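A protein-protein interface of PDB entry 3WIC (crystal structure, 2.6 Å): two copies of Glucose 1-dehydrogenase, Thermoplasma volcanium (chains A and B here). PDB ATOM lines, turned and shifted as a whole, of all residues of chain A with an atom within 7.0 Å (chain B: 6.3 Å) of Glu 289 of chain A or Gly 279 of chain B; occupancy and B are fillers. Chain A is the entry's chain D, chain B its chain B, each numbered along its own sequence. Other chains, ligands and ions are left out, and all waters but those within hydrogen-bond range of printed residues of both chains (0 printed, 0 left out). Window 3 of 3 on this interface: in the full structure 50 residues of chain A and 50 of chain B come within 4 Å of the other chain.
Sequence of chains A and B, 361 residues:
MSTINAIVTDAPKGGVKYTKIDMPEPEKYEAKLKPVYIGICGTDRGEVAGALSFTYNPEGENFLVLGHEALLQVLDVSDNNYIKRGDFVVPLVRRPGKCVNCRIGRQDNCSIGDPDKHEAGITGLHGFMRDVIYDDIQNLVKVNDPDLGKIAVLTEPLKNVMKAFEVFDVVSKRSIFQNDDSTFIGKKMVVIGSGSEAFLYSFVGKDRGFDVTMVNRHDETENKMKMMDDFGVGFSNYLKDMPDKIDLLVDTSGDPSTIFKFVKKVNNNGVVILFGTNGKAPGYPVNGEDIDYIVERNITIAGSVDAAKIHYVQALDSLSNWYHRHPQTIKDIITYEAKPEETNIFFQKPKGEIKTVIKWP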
ATOM      1  N   LYS A 264      15.888   0.589  -2.771  1.00  0.00           N
ATOM      2  CA  LYS A 264      16.681  -0.396  -3.548  1.00  0.00           C
ATOM      3  C   LYS A 264      16.419  -0.378  -5.043  1.00  0.00           C
ATOM      4  O   LYS A 264      17.009  -1.153  -5.793  1.00  0.00           O
ATOM      5  CB  LYS A 264      16.552  -1.810  -2.954  1.00  0.00           C
ATOM      6  CG  LYS A 264      17.403  -2.000  -1.699  1.00  0.00           C
ATOM      7  CD  LYS A 264      17.270  -3.398  -1.122  1.00  0.00           C
ATOM      8  CE  LYS A 264      16.061  -3.530  -0.191  1.00  0.00           C
ATOM      9  NZ  LYS A 264      15.857  -4.963   0.104  1.00  0.00           N
ATOM     10  N   VAL A 286      17.279  -3.461   8.538  1.00  0.00           N
ATOM     11  CA  VAL A 286      18.226  -2.912   7.514  1.00  0.00           C
ATOM     12  C   VAL A 286      19.581  -3.629   7.660  1.00  0.00           C
ATOM     13  O   VAL A 286      20.165  -3.654   8.735  1.00  0.00           O
ATOM     14  CB  VAL A 286      18.375  -1.350   7.593  1.00  0.00           C
ATOM     15  CG1 VAL A 286      19.338  -0.843   6.539  1.00  0.00           C
ATOM     16  CG2 VAL A 286      17.030  -0.642   7.409  1.00  0.00           C
ATOM     17  N   ASN A 287      20.059  -4.235   6.587  1.00  0.00           N
ATOM     18  CA  ASN A 287      21.333  -4.971   6.621  1.00  0.00           C
ATOM     19  C   ASN A 287      22.477  -4.278   5.879  1.00  0.00           C
ATOM     20  O   ASN A 287      22.333  -3.185   5.356  1.00  0.00           O
ATOM     21  CB  ASN A 287      21.118  -6.339   6.023  1.00  0.00           C
ATOM     22  CG  ASN A 287      20.740  -6.260   4.568  1.00  0.00           C
ATOM     23  OD1 ASN A 287      21.237  -5.390   3.844  1.00  0.00           O
ATOM     24  ND2 ASN A 287      19.835  -7.151   4.129  1.00  0.00           N
ATOM     25  N   GLY A 288      23.617  -4.951   5.826  1.00  0.00           N
ATOM     26  CA  GLY A 288      24.835  -4.385   5.320  1.00  0.00           C
ATOM     27  C   GLY A 288      24.799  -4.172   3.848  1.00  0.00           C
ATOM     28  O   GLY A 288      25.631  -3.472   3.289  1.00  0.00           O
ATOM     29  N   GLU A 289      23.851  -4.789   3.191  1.00  0.00           N
ATOM     30  CA  GLU A 289      23.748  -4.610   1.763  1.00  0.00           C
ATOM     31  C   GLU A 289      22.941  -3.362   1.483  1.00  0.00           C
ATOM     32  O   GLU A 289      23.227  -2.614   0.579  1.00  0.00           O
ATOM     33  CB  GLU A 289      23.105  -5.830   1.140  1.00  0.00           C
ATOM     34  CG  GLU A 289      24.020  -7.023   1.162  1.00  0.00           C
ATOM     35  CD  GLU A 289      23.355  -8.199   0.487  1.00  0.00           C
ATOM     36  OE1 GLU A 289      22.247  -8.573   0.942  1.00  0.00           O
ATOM     37  OE2 GLU A 289      23.907  -8.720  -0.510  1.00  0.00           O
ATOM     38  N   ASP A 290      21.911  -3.152   2.271  1.00  0.00           N
ATOM     39  CA  ASP A 290      21.132  -1.941   2.169  1.00  0.00           C
ATOM     40  C   ASP A 290      22.003  -0.706   2.331  1.00  0.00           C
ATOM     41  O   ASP A 290      21.831   0.265   1.604  1.00  0.00           O
ATOM     42  CB  ASP A 290      20.030  -1.937   3.217  1.00  0.00           C
ATOM     43  CG  ASP A 290      19.187  -3.198   3.181  1.00  0.00           C
ATOM     44  OD1 ASP A 290      19.101  -3.817   2.086  1.00  0.00           O
ATOM     45  OD2 ASP A 290      18.636  -3.571   4.257  1.00  0.00           O
ATOM     46  N   ILE A 291      22.927  -0.755   3.303  1.00  0.00           N
ATOM     47  CA  ILE A 291      23.814   0.351   3.556  1.00  0.00           C
ATOM     48  C   ILE A 291      24.777   0.529   2.390  1.00  0.00           C
ATOM     49  O   ILE A 291      25.028   1.671   1.927  1.00  0.00           O
ATOM     50  CB  ILE A 291      24.581   0.181   4.862  1.00  0.00           C
ATOM     51  CG1 ILE A 291      23.607   0.233   6.050  1.00  0.00           C
ATOM     52  CG2 ILE A 291      25.662   1.280   4.988  1.00  0.00           C
ATOM     53  CD1 ILE A 291      22.782   1.523   6.175  1.00  0.00           C
ATOM     54  N   ASP A 292      25.271  -0.600   1.896  1.00  0.00           N
ATOM     55  CA  ASP A 292      26.216  -0.579   0.815  1.00  0.00           C
ATOM     56  C   ASP A 292      25.621  -0.020  -0.488  1.00  0.00           C
ATOM     57  O   ASP A 292      26.250   0.762  -1.205  1.00  0.00           O
ATOM     58  CB  ASP A 292      26.718  -1.973   0.562  1.00  0.00           C
ATOM     59  CG  ASP A 292      27.605  -2.023  -0.615  1.00  0.00           C
ATOM     60  OD1 ASP A 292      28.679  -1.404  -0.569  1.00  0.00           O
ATOM     61  OD2 ASP A 292      27.203  -2.621  -1.621  1.00  0.00           O
ATOM     62  N   TYR A 293      24.405  -0.459  -0.783  1.00  0.00           N
ATOM     63  CA  TYR A 293      23.629   0.071  -1.874  1.00  0.00           C
ATOM     64  C   TYR A 293      23.640   1.638  -1.820  1.00  0.00           C
ATOM     65  O   TYR A 293      24.094   2.318  -2.718  1.00  0.00           O
ATOM     66  CB  TYR A 293      22.201  -0.505  -1.795  1.00  0.00           C
ATOM     67  CG  TYR A 293      21.363  -0.175  -3.006  1.00  0.00           C
ATOM     68  CD1 TYR A 293      20.697   1.051  -3.095  1.00  0.00           C
ATOM     69  CD2 TYR A 293      21.243  -1.063  -4.060  1.00  0.00           C
ATOM     70  CE1 TYR A 293      19.943   1.395  -4.213  1.00  0.00           C
ATOM     71  CE2 TYR A 293      20.476  -0.742  -5.188  1.00  0.00           C
ATOM     72  CZ  TYR A 293      19.834   0.499  -5.264  1.00  0.00           C
ATOM     73  OH  TYR A 293      19.077   0.865  -6.362  1.00  0.00           O
ATOM     74  N   ILE A 294      23.182   2.163  -0.708  1.00  0.00           N
ATOM     75  CA  ILE A 294      23.097   3.569  -0.520  1.00  0.00           C
ATOM     76  C   ILE A 294      24.466   4.218  -0.697  1.00  0.00           C
ATOM     77  O   ILE A 294      24.578   5.261  -1.343  1.00  0.00           O
ATOM     78  CB  ILE A 294      22.529   3.895   0.865  1.00  0.00           C
ATOM     79  CG1 ILE A 294      21.069   3.437   0.945  1.00  0.00           C
ATOM     80  CG2 ILE A 294      22.692   5.377   1.158  1.00  0.00           C
ATOM     81  CD1 ILE A 294      20.501   3.446   2.362  1.00  0.00           C
ATOM     82  N   VAL A 295      25.494   3.587  -0.144  1.00  0.00           N
ATOM     83  CA  VAL A 295      26.844   4.115  -0.267  1.00  0.00           C
ATOM     84  C   VAL A 295      27.349   4.151  -1.723  1.00  0.00           C
ATOM     85  O   VAL A 295      27.824   5.182  -2.169  1.00  0.00           O
ATOM     86  CB  VAL A 295      27.836   3.343   0.641  1.00  0.00           C
ATOM     87  CG1 VAL A 295      29.266   3.754   0.354  1.00  0.00           C
ATOM     88  CG2 VAL A 295      27.538   3.606   2.115  1.00  0.00           C
ATOM     89  N   GLY B 254      30.099   0.424   8.539  1.00  0.00           N
ATOM     90  CA  GLY B 254      29.164  -0.295   7.677  1.00  0.00           C
ATOM     91  C   GLY B 254      28.147  -1.133   8.447  1.00  0.00           C
ATOM     92  O   GLY B 254      27.386  -1.900   7.840  1.00  0.00           O
ATOM     93  N   THR B 277      31.453   0.220   4.471  1.00  0.00           N
ATOM     94  CA  THR B 277      30.568  -0.841   3.954  1.00  0.00           C
ATOM     95  C   THR B 277      30.947  -2.250   4.436  1.00  0.00           C
ATOM     96  O   THR B 277      32.106  -2.595   4.591  1.00  0.00           O
ATOM     97  CB  THR B 277      30.547  -0.865   2.415  1.00  0.00           C
ATOM     98  OG1 THR B 277      31.855  -1.166   1.882  1.00  0.00           O
ATOM     99  CG2 THR B 277      30.044   0.483   1.873  1.00  0.00           C
ATOM    100  N   ASN B 278      29.934  -3.059   4.685  1.00  0.00           N
ATOM    101  CA  ASN B 278      30.123  -4.444   5.027  1.00  0.00           C
ATOM    102  C   ASN B 278      28.860  -5.203   4.668  1.00  0.00           C
ATOM    103  O   ASN B 278      27.873  -5.170   5.407  1.00  0.00           O
ATOM    104  CB  ASN B 278      30.446  -4.583   6.511  1.00  0.00           C
ATOM    105  CG  ASN B 278      30.692  -6.036   6.932  1.00  0.00           C
ATOM    106  OD1 ASN B 278      30.995  -6.896   6.105  1.00  0.00           O
ATOM    107  ND2 ASN B 278      30.557  -6.305   8.221  1.00  0.00           N
ATOM    108  N   GLY B 279      28.934  -5.885   3.534  1.00  0.00           N
ATOM    109  CA  GLY B 279      27.885  -6.778   3.015  1.00  0.00           C
ATOM    110  C   GLY B 279      27.338  -7.833   3.948  1.00  0.00           C
ATOM    111  O   GLY B 279      26.184  -8.253   3.783  1.00  0.00           O
ATOM    112  N   LYS B 280      28.127  -8.232   4.949  1.00  0.00           N
ATOM    113  CA  LYS B 280      27.728  -9.305   5.870  1.00  0.00           C
ATOM    114  C   LYS B 280      27.058  -8.814   7.162  1.00  0.00           C
ATOM    115  O   LYS B 280      26.544  -9.615   7.963  1.00  0.00           O
ATOM    116  CB  LYS B 280      28.947 -10.169   6.205  1.00  0.00           C
ATOM    117  CG  LYS B 280      29.603 -10.763   4.973  1.00  0.00           C
ATOM    118  CD  LYS B 280      31.002 -11.276   5.272  1.00  0.00           C
ATOM    119  CE  LYS B 280      31.986 -10.153   5.613  1.00  0.00           C
ATOM    120  NZ  LYS B 280      32.275  -9.199   4.495  1.00  0.00           N
ATOM    121  N   ALA B 281      27.066  -7.510   7.381  1.00  0.00           N
ATOM    122  CA  ALA B 281      26.598  -6.973   8.665  1.00  0.00           C
ATOM    123  C   ALA B 281      25.155  -7.396   8.916  1.00  0.00           C
ATOM    124  O   ALA B 281      24.322  -7.294   8.012  1.00  0.00           O
ATOM    125  CB  ALA B 281      26.715  -5.450   8.681  1.00  0.00           C
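No position is printed for both chains.
Of the 11 printed residues of chain A, 5 touch a printed residue of chain B. Hydrophobic or aromatic side chains of chain A that line the printed part of chain B: Val 295. Printed residues of chain B that touch a printed residue of chain A: Thr 277, Asn 278, Gly 279 and Ala 281. Among the printed residues, 6 pairs touch across the chains.
The backbone carbonyl oxygen (O) of Ala 281 of chain B lies within hydrogen-bond range of the backbone NH (N) of Gly 288 of chain A, at 3.3 Å.
Glu 289 of chain A touches one residue of chain B. Of the printed residues of chain A, Gly 279 of chain B touches Glu 289. Printed residues of chain A within 4 Å of Asn 278 of chain B: Gly 288. Of the printed residues of chain B, Val 295 of chain A touches Thr 277 (3.7 Å). Printed residues of chain B within 4 Å of Gly 288 of chain A: Asn 278 (3.1 Å) and Ala 281 (3.3 Å). Printed residues of chain A within 4 Å of Ala 281 of chain B: Asn 287 and Gly 288. The nearest printed residue of chain A that does not touch Gly 279 of chain B is Gly 288 of chain A (4.01 Å).
NZ of Lys 280 of chain B sits at hydrogen-bond distance from OD1 of Asn 278 of chain B, 3.1 Å away. The side-chain amide oxygen (OD1) of Asn 287 of chain A lies within hydrogen-bond range of the backbone NH (N) of Glu 289 of chain A (2.8 Å). The backbone NH (N) of Asn 287 of chain A lies within hydrogen-bond range of the side-chain carboxylate (OD2) of Asp 290 of chain A.
Among the printed residues, pairs that only touch across the chains: Gly 288 of chain A with Asn 278 of chain B, Asp 292 of chain A with Thr 277 of chain B, Glu 289 of chain A with Gly 279 of chain B, Val 295 of chain A with Thr 277 of chain B and Asn 287 of chain A with Ala 281 of chain B.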
